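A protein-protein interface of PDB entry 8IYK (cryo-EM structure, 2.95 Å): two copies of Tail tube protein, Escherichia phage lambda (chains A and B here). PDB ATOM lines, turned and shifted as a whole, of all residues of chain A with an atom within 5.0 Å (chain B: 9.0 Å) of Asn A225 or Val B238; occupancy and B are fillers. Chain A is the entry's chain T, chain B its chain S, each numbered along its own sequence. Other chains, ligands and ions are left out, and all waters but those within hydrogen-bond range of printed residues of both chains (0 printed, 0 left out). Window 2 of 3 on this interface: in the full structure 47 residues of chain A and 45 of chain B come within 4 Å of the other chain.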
ATOM      1  N   VAL A 198       5.011   2.400  27.554  1.00  0.00           N
ATOM      2  CA  VAL A 198       3.677   2.718  27.057  1.00  0.00           C
ATOM      3  C   VAL A 198       3.282   1.642  26.052  1.00  0.00           C
ATOM      4  O   VAL A 198       4.091   0.798  25.669  1.00  0.00           O
ATOM      5  CB  VAL A 198       3.617   4.134  26.435  1.00  0.00           C
ATOM      6  CG1 VAL A 198       4.047   4.102  24.988  1.00  0.00           C
ATOM      7  CG2 VAL A 198       2.224   4.736  26.583  1.00  0.00           C
ATOM      8  N   SER A 199       2.016   1.654  25.639  1.00  0.00           N
ATOM      9  CA  SER A 199       1.494   0.655  24.718  1.00  0.00           C
ATOM     10  C   SER A 199       1.764   1.084  23.276  1.00  0.00           C
ATOM     11  O   SER A 199       2.447   2.078  23.015  1.00  0.00           O
ATOM     12  CB  SER A 199       0.006   0.427  24.976  1.00  0.00           C
ATOM     13  OG  SER A 199      -0.670   0.074  23.783  1.00  0.00           O
ATOM     14  N   ALA A 200       1.226   0.328  22.315  1.00  0.00           N
ATOM     15  CA  ALA A 200       1.394   0.636  20.902  1.00  0.00           C
ATOM     16  C   ALA A 200       0.143   1.194  20.241  1.00  0.00           C
ATOM     17  O   ALA A 200       0.251   1.810  19.177  1.00  0.00           O
ATOM     18  CB  ALA A 200       1.845  -0.613  20.129  1.00  0.00           C
ATOM     19  N   ASP A 201      -1.034   0.984  20.828  1.00  0.00           N
ATOM     20  CA  ASP A 201      -2.269   1.561  20.310  1.00  0.00           C
ATOM     21  C   ASP A 201      -3.137   2.220  21.371  1.00  0.00           C
ATOM     22  O   ASP A 201      -3.975   3.057  21.012  1.00  0.00           O
ATOM     23  CB  ASP A 201      -3.102   0.492  19.586  1.00  0.00           C
ATOM     24  CG  ASP A 201      -3.542  -0.627  20.506  1.00  0.00           C
ATOM     25  OD1 ASP A 201      -2.936  -0.785  21.586  1.00  0.00           O
ATOM     26  OD2 ASP A 201      -4.499  -1.345  20.152  1.00  0.00           O
ATOM     27  N   LYS A 223      -4.359  -9.022  20.665  1.00  0.00           N
ATOM     28  CA  LYS A 223      -2.931  -8.971  20.953  1.00  0.00           C
ATOM     29  C   LYS A 223      -2.480  -7.517  20.941  1.00  0.00           C
ATOM     30  O   LYS A 223      -2.680  -6.810  19.947  1.00  0.00           O
ATOM     31  CB  LYS A 223      -2.138  -9.790  19.933  1.00  0.00           C
ATOM     32  CG  LYS A 223      -0.643  -9.846  20.209  1.00  0.00           C
ATOM     33  CD  LYS A 223       0.135  -8.968  19.240  1.00  0.00           C
ATOM     34  CE  LYS A 223       1.617  -9.306  19.257  1.00  0.00           C
ATOM     35  NZ  LYS A 223       2.329  -8.747  18.074  1.00  0.00           N
ATOM     36  N   VAL A 224      -1.870  -7.075  22.038  1.00  0.00           N
ATOM     37  CA  VAL A 224      -1.419  -5.700  22.187  1.00  0.00           C
ATOM     38  C   VAL A 224       0.083  -5.702  22.429  1.00  0.00           C
ATOM     39  O   VAL A 224       0.650  -6.657  22.973  1.00  0.00           O
ATOM     40  CB  VAL A 224      -2.169  -4.972  23.328  1.00  0.00           C
ATOM     41  CG1 VAL A 224      -1.614  -5.372  24.686  1.00  0.00           C
ATOM     42  CG2 VAL A 224      -2.104  -3.466  23.139  1.00  0.00           C
ATOM     43  N   ASN A 225       0.732  -4.620  22.003  1.00  0.00           N
ATOM     44  CA  ASN A 225       2.175  -4.463  22.106  1.00  0.00           C
ATOM     45  C   ASN A 225       2.490  -3.294  23.026  1.00  0.00           C
ATOM     46  O   ASN A 225       1.898  -2.218  22.897  1.00  0.00           O
ATOM     47  CB  ASN A 225       2.802  -4.241  20.726  1.00  0.00           C
ATOM     48  CG  ASN A 225       2.793  -5.495  19.874  1.00  0.00           C
ATOM     49  OD1 ASN A 225       1.803  -5.799  19.207  1.00  0.00           O
ATOM     50  ND2 ASN A 225       3.899  -6.229  19.888  1.00  0.00           N
ATOM     51  N   ILE A 226       3.415  -3.513  23.954  1.00  0.00           N
ATOM     52  CA  ILE A 226       3.845  -2.491  24.905  1.00  0.00           C
ATOM     53  C   ILE A 226       5.328  -2.219  24.686  1.00  0.00           C
ATOM     54  O   ILE A 226       6.171  -3.068  25.015  1.00  0.00           O
ATOM     55  CB  ILE A 226       3.554  -2.921  26.351  1.00  0.00           C
ATOM     56  CG1 ILE A 226       2.045  -2.991  26.587  1.00  0.00           C
ATOM     57  CG2 ILE A 226       4.203  -1.962  27.340  1.00  0.00           C
ATOM     58  CD1 ILE A 226       1.511  -4.400  26.695  1.00  0.00           C
ATOM     59  N   PRO A 227       5.684  -1.092  24.071  1.00  0.00           N
ATOM     60  CA  PRO A 227       7.096  -0.701  23.999  1.00  0.00           C
ATOM     61  C   PRO A 227       7.574   0.039  25.242  1.00  0.00           C
ATOM     62  O   PRO A 227       6.873   0.883  25.812  1.00  0.00           O
ATOM     63  CB  PRO A 227       7.145   0.213  22.767  1.00  0.00           C
ATOM     64  CG  PRO A 227       5.751   0.690  22.585  1.00  0.00           C
ATOM     65  CD  PRO A 227       4.872  -0.428  23.038  1.00  0.00           C
ATOM     66  N   VAL A 238      10.083  -4.907  24.070  1.00  0.00           N
ATOM     67  CA  VAL A 238       8.747  -5.034  23.502  1.00  0.00           C
ATOM     68  C   VAL A 238       8.040  -6.181  24.206  1.00  0.00           C
ATOM     69  O   VAL A 238       8.571  -7.295  24.271  1.00  0.00           O
ATOM     70  CB  VAL A 238       8.795  -5.276  21.980  1.00  0.00           C
ATOM     71  CG1 VAL A 238       7.505  -5.926  21.500  1.00  0.00           C
ATOM     72  CG2 VAL A 238       9.052  -3.972  21.243  1.00  0.00           C
ATOM     73  N   ALA A 239       6.849  -5.913  24.733  1.00  0.00           N
ATOM     74  CA  ALA A 239       6.046  -6.928  25.399  1.00  0.00           C
ATOM     75  C   ALA A 239       4.780  -7.194  24.598  1.00  0.00           C
ATOM     76  O   ALA A 239       4.180  -6.268  24.046  1.00  0.00           O
ATOM     77  CB  ALA A 239       5.683  -6.499  26.823  1.00  0.00           C
ATOM     78  N   GLU A 240       4.379  -8.459  24.529  1.00  0.00           N
ATOM     79  CA  GLU A 240       3.145  -8.858  23.868  1.00  0.00           C
ATOM     80  C   GLU A 240       2.169  -9.376  24.914  1.00  0.00           C
ATOM     81  O   GLU A 240       2.499 -10.289  25.677  1.00  0.00           O
ATOM     82  CB  GLU A 240       3.409  -9.928  22.805  1.00  0.00           C
ATOM     83  CG  GLU A 240       4.480 -10.936  23.184  1.00  0.00           C
ATOM     84  CD  GLU A 240       5.127 -11.582  21.975  1.00  0.00           C
ATOM     85  OE1 GLU A 240       4.390 -11.979  21.048  1.00  0.00           O
ATOM     86  OE2 GLU A 240       6.370 -11.694  21.952  1.00  0.00           O
ATOM     87  N   MET B 164      -0.731   8.673  14.933  1.00  0.00           N
ATOM     88  CA  MET B 164       0.336   8.292  14.018  1.00  0.00           C
ATOM     89  C   MET B 164       0.279   6.786  13.814  1.00  0.00           C
ATOM     90  O   MET B 164      -0.340   6.059  14.596  1.00  0.00           O
ATOM     91  CB  MET B 164       1.718   8.706  14.533  1.00  0.00           C
ATOM     92  CG  MET B 164       2.084   8.139  15.891  1.00  0.00           C
ATOM     93  SD  MET B 164       3.826   7.668  15.928  1.00  0.00           S
ATOM     94  CE  MET B 164       3.919   6.798  17.487  1.00  0.00           C
ATOM     95  N   THR B 165       0.936   6.328  12.752  1.00  0.00           N
ATOM     96  CA  THR B 165       1.017   4.908  12.442  1.00  0.00           C
ATOM     97  C   THR B 165       2.436   4.577  12.007  1.00  0.00           C
ATOM     98  O   THR B 165       3.190   5.448  11.572  1.00  0.00           O
ATOM     99  CB  THR B 165       0.023   4.504  11.344  1.00  0.00           C
ATOM    100  OG1 THR B 165       0.075   5.455  10.274  1.00  0.00           O
ATOM    101  CG2 THR B 165      -1.394   4.444  11.897  1.00  0.00           C
ATOM    102  N   VAL B 166       2.802   3.305  12.138  1.00  0.00           N
ATOM    103  CA  VAL B 166       4.112   2.818  11.722  1.00  0.00           C
ATOM    104  C   VAL B 166       3.897   1.602  10.833  1.00  0.00           C
ATOM    105  O   VAL B 166       3.458   0.548  11.309  1.00  0.00           O
ATOM    106  CB  VAL B 166       5.013   2.469  12.915  1.00  0.00           C
ATOM    107  CG1 VAL B 166       6.318   1.858  12.430  1.00  0.00           C
ATOM    108  CG2 VAL B 166       5.288   3.710  13.749  1.00  0.00           C
ATOM    109  N   THR B 167       4.200   1.746   9.546  1.00  0.00           N
ATOM    110  CA  THR B 167       4.127   0.640   8.601  1.00  0.00           C
ATOM    111  C   THR B 167       5.541   0.202   8.244  1.00  0.00           C
ATOM    112  O   THR B 167       6.271   0.957   7.579  1.00  0.00           O
ATOM    113  CB  THR B 167       3.356   1.041   7.343  1.00  0.00           C
ATOM    114  OG1 THR B 167       2.038   1.472   7.704  1.00  0.00           O
ATOM    115  CG2 THR B 167       3.256  -0.134   6.383  1.00  0.00           C
ATOM    116  N   PRO B 168       5.978  -0.971   8.683  1.00  0.00           N
ATOM    117  CA  PRO B 168       7.304  -1.470   8.319  1.00  0.00           C
ATOM    118  C   PRO B 168       7.241  -2.378   7.095  1.00  0.00           C
ATOM    119  O   PRO B 168       6.171  -2.787   6.641  1.00  0.00           O
ATOM    120  CB  PRO B 168       7.713  -2.264   9.562  1.00  0.00           C
ATOM    121  CG  PRO B 168       6.409  -2.818  10.069  1.00  0.00           C
ATOM    122  CD  PRO B 168       5.311  -1.856   9.653  1.00  0.00           C
ATOM    123  N   SER B 170       8.627  -5.412   7.257  1.00  0.00           N
ATOM    124  CA  SER B 170       8.360  -6.700   7.901  1.00  0.00           C
ATOM    125  C   SER B 170       8.778  -7.866   7.005  1.00  0.00           C
ATOM    126  O   SER B 170       8.073  -8.870   6.879  1.00  0.00           O
ATOM    127  CB  SER B 170       6.889  -6.818   8.311  1.00  0.00           C
ATOM    128  OG  SER B 170       6.084  -7.218   7.217  1.00  0.00           O
ATOM    129  N   LEU B 181      11.904   1.487   6.952  1.00  0.00           N
ATOM    130  CA  LEU B 181      10.635   1.481   7.666  1.00  0.00           C
ATOM    131  C   LEU B 181       9.921   2.810   7.458  1.00  0.00           C
ATOM    132  O   LEU B 181      10.562   3.860   7.358  1.00  0.00           O
ATOM    133  CB  LEU B 181      10.851   1.228   9.159  1.00  0.00           C
ATOM    134  CG  LEU B 181      10.715  -0.219   9.637  1.00  0.00           C
ATOM    135  CD1 LEU B 181      11.947  -1.027   9.266  1.00  0.00           C
ATOM    136  CD2 LEU B 181      10.469  -0.268  11.137  1.00  0.00           C
ATOM    137  N   ALA B 197      13.206   5.692  17.260  1.00  0.00           N
ATOM    138  CA  ALA B 197      13.045   4.245  17.249  1.00  0.00           C
ATOM    139  C   ALA B 197      14.321   3.593  17.754  1.00  0.00           C
ATOM    140  O   ALA B 197      15.423   3.971  17.345  1.00  0.00           O
ATOM    141  CB  ALA B 197      12.716   3.729  15.845  1.00  0.00           C
ATOM    142  N   VAL B 198      14.173   2.615  18.645  1.00  0.00           N
ATOM    143  CA  VAL B 198      15.324   1.956  19.256  1.00  0.00           C
ATOM    144  C   VAL B 198      15.071   0.457  19.288  1.00  0.00           C
ATOM    145  O   VAL B 198      13.995   0.017  19.702  1.00  0.00           O
ATOM    146  CB  VAL B 198      15.606   2.492  20.674  1.00  0.00           C
ATOM    147  CG1 VAL B 198      14.303   2.830  21.384  1.00  0.00           C
ATOM    148  CG2 VAL B 198      16.424   1.490  21.479  1.00  0.00           C
ATOM    149  N   ALA B 200      14.813  -3.313  20.341  1.00  0.00           N
ATOM    150  CA  ALA B 200      14.497  -3.921  21.626  1.00  0.00           C
ATOM    151  C   ALA B 200      15.471  -5.020  22.025  1.00  0.00           C
ATOM    152  O   ALA B 200      15.359  -5.550  23.135  1.00  0.00           O
ATOM    153  CB  ALA B 200      13.074  -4.485  21.607  1.00  0.00           C
ATOM    154  N   VAL B 224      13.763  -9.574  14.946  1.00  0.00           N
ATOM    155  CA  VAL B 224      14.021  -8.369  15.722  1.00  0.00           C
ATOM    156  C   VAL B 224      12.734  -7.568  15.857  1.00  0.00           C
ATOM    157  O   VAL B 224      11.893  -7.538  14.948  1.00  0.00           O
ATOM    158  CB  VAL B 224      15.147  -7.535  15.079  1.00  0.00           C
ATOM    159  CG1 VAL B 224      14.681  -6.880  13.791  1.00  0.00           C
ATOM    160  CG2 VAL B 224      15.648  -6.483  16.048  1.00  0.00           C
ATOM    161  N   ASN B 225      12.564  -6.938  17.016  1.00  0.00           N
ATOM    162  CA  ASN B 225      11.428  -6.069  17.292  1.00  0.00           C
ATOM    163  C   ASN B 225      11.952  -4.657  17.502  1.00  0.00           C
ATOM    164  O   ASN B 225      12.810  -4.432  18.363  1.00  0.00           O
ATOM    165  CB  ASN B 225      10.649  -6.550  18.518  1.00  0.00           C
ATOM    166  CG  ASN B 225      10.282  -8.017  18.434  1.00  0.00           C
ATOM    167  OD1 ASN B 225      11.056  -8.886  18.835  1.00  0.00           O
ATOM    168  ND2 ASN B 225       9.094  -8.302  17.913  1.00  0.00           N
ATOM    169  N   ILE B 226      11.443  -3.717  16.717  1.00  0.00           N
ATOM    170  CA  ILE B 226      11.849  -2.318  16.773  1.00  0.00           C
ATOM    171  C   ILE B 226      10.690  -1.517  17.367  1.00  0.00           C
ATOM    172  O   ILE B 226       9.637  -1.373  16.724  1.00  0.00           O
ATOM    173  CB  ILE B 226      12.259  -1.791  15.390  1.00  0.00           C
ATOM    174  CG1 ILE B 226      12.385  -0.266  15.404  1.00  0.00           C
ATOM    175  CG2 ILE B 226      11.309  -2.286  14.302  1.00  0.00           C
ATOM    176  CD1 ILE B 226      13.540   0.232  16.234  1.00  0.00           C
ATOM    177  N   PRO B 227      10.805  -1.046  18.608  1.00  0.00           N
ATOM    178  CA  PRO B 227       9.825  -0.094  19.141  1.00  0.00           C
ATOM    179  C   PRO B 227      10.180   1.357  18.848  1.00  0.00           C
ATOM    180  O   PRO B 227      11.334   1.787  18.947  1.00  0.00           O
ATOM    181  CB  PRO B 227       9.862  -0.370  20.650  1.00  0.00           C
ATOM    182  CG  PRO B 227      11.199  -0.949  20.900  1.00  0.00           C
ATOM    183  CD  PRO B 227      11.551  -1.732  19.675  1.00  0.00           C
ATOM    184  N   VAL B 228       9.143   2.119  18.502  1.00  0.00           N
ATOM    185  CA  VAL B 228       9.244   3.533  18.170  1.00  0.00           C
ATOM    186  C   VAL B 228       8.348   4.311  19.124  1.00  0.00           C
ATOM    187  O   VAL B 228       7.238   3.871  19.438  1.00  0.00           O
ATOM    188  CB  VAL B 228       8.833   3.803  16.707  1.00  0.00           C
ATOM    189  CG1 VAL B 228       9.383   5.136  16.237  1.00  0.00           C
ATOM    190  CG2 VAL B 228       9.286   2.667  15.801  1.00  0.00           C
ATOM    191  N   VAL B 229       8.833   5.460  19.588  1.00  0.00           N
ATOM    192  CA  VAL B 229       8.094   6.333  20.493  1.00  0.00           C
ATOM    193  C   VAL B 229       8.157   7.750  19.939  1.00  0.00           C
ATOM    194  O   VAL B 229       9.234   8.223  19.560  1.00  0.00           O
ATOM    195  CB  VAL B 229       8.661   6.279  21.925  1.00  0.00           C
ATOM    196  CG1 VAL B 229       8.027   7.344  22.793  1.00  0.00           C
ATOM    197  CG2 VAL B 229       8.443   4.901  22.529  1.00  0.00           C
ATOM    198  N   PHE B 235       2.601   8.839  22.042  1.00  0.00           N
ATOM    199  CA  PHE B 235       2.236   7.678  21.244  1.00  0.00           C
ATOM    200  C   PHE B 235       3.467   6.820  20.983  1.00  0.00           C
ATOM    201  O   PHE B 235       4.608   7.283  21.072  1.00  0.00           O
ATOM    202  CB  PHE B 235       1.599   8.088  19.904  1.00  0.00           C
ATOM    203  CG  PHE B 235       0.106   8.263  19.961  1.00  0.00           C
ATOM    204  CD1 PHE B 235      -0.550   8.388  21.173  1.00  0.00           C
ATOM    205  CD2 PHE B 235      -0.642   8.297  18.797  1.00  0.00           C
ATOM    206  CE1 PHE B 235      -1.922   8.550  21.224  1.00  0.00           C
ATOM    207  CE2 PHE B 235      -2.015   8.456  18.841  1.00  0.00           C
ATOM    208  CZ  PHE B 235      -2.655   8.583  20.056  1.00  0.00           C
ATOM    209  N   ALA B 236       3.220   5.555  20.653  1.00  0.00           N
ATOM    210  CA  ALA B 236       4.294   4.617  20.352  1.00  0.00           C
ATOM    211  C   ALA B 236       3.739   3.487  19.499  1.00  0.00           C
ATOM    212  O   ALA B 236       2.525   3.335  19.342  1.00  0.00           O
ATOM    213  CB  ALA B 236       4.939   4.073  21.628  1.00  0.00           C
ATOM    214  N   ALA B 237       4.653   2.696  18.942  1.00  0.00           N
ATOM    215  CA  ALA B 237       4.296   1.563  18.103  1.00  0.00           C
ATOM    216  C   ALA B 237       5.429   0.546  18.122  1.00  0.00           C
ATOM    217  O   ALA B 237       6.546   0.837  18.558  1.00  0.00           O
ATOM    218  CB  ALA B 237       3.988   1.997  16.666  1.00  0.00           C
ATOM    219  N   VAL B 238       5.121  -0.661  17.651  1.00  0.00           N
ATOM    220  CA  VAL B 238       6.067  -1.770  17.618  1.00  0.00           C
ATOM    221  C   VAL B 238       6.038  -2.385  16.227  1.00  0.00           C
ATOM    222  O   VAL B 238       4.958  -2.623  15.675  1.00  0.00           O
ATOM    223  CB  VAL B 238       5.737  -2.830  18.688  1.00  0.00           C
ATOM    224  CG1 VAL B 238       6.530  -4.106  18.445  1.00  0.00           C
ATOM    225  CG2 VAL B 238       6.006  -2.282  20.079  1.00  0.00           C
ATOM    226  N   ALA B 239       7.217  -2.638  15.659  1.00  0.00           N
ATOM    227  CA  ALA B 239       7.329  -3.284  14.361  1.00  0.00           C
ATOM    228  C   ALA B 239       8.239  -4.499  14.477  1.00  0.00           C
ATOM    229  O   ALA B 239       9.057  -4.599  15.392  1.00  0.00           O
ATOM    230  CB  ALA B 239       7.865  -2.319  13.297  1.00  0.00           C
ATOM    231  N   GLU B 240       8.081  -5.432  13.543  1.00  0.00           N
ATOM    232  CA  GLU B 240       8.863  -6.661  13.518  1.00  0.00           C
ATOM    233  C   GLU B 240       9.588  -6.789  12.188  1.00  0.00           C
ATOM    234  O   GLU B 240       9.025  -6.486  11.130  1.00  0.00           O
ATOM    235  CB  GLU B 240       7.975  -7.889  13.746  1.00  0.00           C
ATOM    236  CG  GLU B 240       8.747  -9.167  14.038  1.00  0.00           C
ATOM    237  CD  GLU B 240       9.032  -9.977  12.787  1.00  0.00           C
ATOM    238  OE1 GLU B 240       8.475  -9.645  11.720  1.00  0.00           O
ATOM    239  OE2 GLU B 240       9.817 -10.946  12.869  1.00  0.00           O
ATOM    240  N   ILE B 241      10.843  -7.237  12.243  1.00  0.00           N
ATOM    241  CA  ILE B 241      11.640  -7.480  11.046  1.00  0.00           C
ATOM    242  C   ILE B 241      12.332  -8.828  11.203  1.00  0.00           C
ATOM    243  O   ILE B 241      13.036  -9.056  12.192  1.00  0.00           O
ATOM    244  CB  ILE B 241      12.676  -6.370  10.797  1.00  0.00           C
ATOM    245  CG1 ILE B 241      12.003  -5.135  10.196  1.00  0.00           C
ATOM    246  CG2 ILE B 241      13.791  -6.865   9.888  1.00  0.00           C
ATOM    247  CD1 ILE B 241      11.710  -5.255   8.716  1.00  0.00           C
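Printed residues of chain A that touch a printed residue of chain B: Val A198, Ser A199, Ala A200, Asn A225, Pro A227 and Val A238.
Hydrophobic or aromatic side chains of chain A that line the printed part of chain B: Val A198, Ala A200, Pro A227 and Val A238.
Among the printed residues, no Asp or Glu carboxylate lies within 4 Å of a Lys or Arg side-chain nitrogen of the other chain.
Among the printed residues, pairs that only touch across the chains: Val A198 with Ala B236 (3.5 Å), Ser A199 with Ala B236 (3.5 Å), Ala A200 with Ala B237 (3.9 Å), Asn A225 with Val B238 (3.7 Å), Pro A227 with Pro B227 (3.5 Å), Pro A227 with Ala B236 (3.6 Å), Pro A227 with Val B238 (3.7 Å), Val A238 with Ala B200 (3.9 Å), Val A238 with Pro B227 (3.7 Å) and Val A238 with Val B238 (3.7 Å).
Printed residues of chain B within 4 Å of Asn A225: Val B238 (3.7 Å).
Val B238 touches just these residues of chain A: Asn A225 (3.7 Å), Pro A227 (3.7 Å) and Val A238 (3.7 Å).
No residue of chain B comes within 4 Å of Val A224.
Ile A226 touches none of the printed residues of chain B.
Of the printed residues of chain B, Pro A227 touches Pro B227, Ala B236 and Val B238.
Of the printed residues of chain A, Ala B200 touches Val A238 (3.9 Å).
Of the printed residues of chain A, Ala B237 touches Ala A200.
Of the printed residues of chain B, Val A238 touches Ala B200 (3.9 Å), Pro B227 (3.7 Å) and Val B238 (3.7 Å).
The nearest residue of chain B that does not touch Asn A225 is Asn B225 (5.9 Å).
The nearest residue of chain A that does not touch Val B238 is Ala A200 (4.1 Å).
The nearest printed residue of chain B that does not touch Val A238 is Asn B225 (4.1 Å).
Asn A225 touches Val B238, but with the chains exchanged Val A238 does not touch Asn B225 (4.1 Å).
Pro A227 touches its own counterpart, Pro B227.
Pro A227 touches Val B238, and with the chains exchanged Val A238 touches Pro B227.
Val A238 touches Ala B200, but with the chains exchanged Ala A200 does not touch Val B238 (4.1 Å).
Of the 11 pairs that touch across the chains among the printed residues, 4 have their exchanged pair printed and touching as well.
The backbone carbonyl oxygen (O) of Ala B236 lies close to the backbone carbonyl oxygen (O) of Ala A200 (2.7 Å).
The backbone NH of Ala B200 lies within hydrogen-bond range of the backbone carbonyl oxygen of Asn B225, 3.0 Å away.
O of Val B228 sits at hydrogen-bond distance from N of Ala B237.
O of Pro A227 lies within hydrogen-bond range of N of Val A198.
N of Asp A201 is in hydrogen-bond range of OG of Ser A199, at 3.1 Å.
N of Ala A200 is in hydrogen-bond range of O of Asn A225 (2.7 Å).
NZ of Lys A223 is in hydrogen-bond range of OD1 of Asn A225 (3.2 Å).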
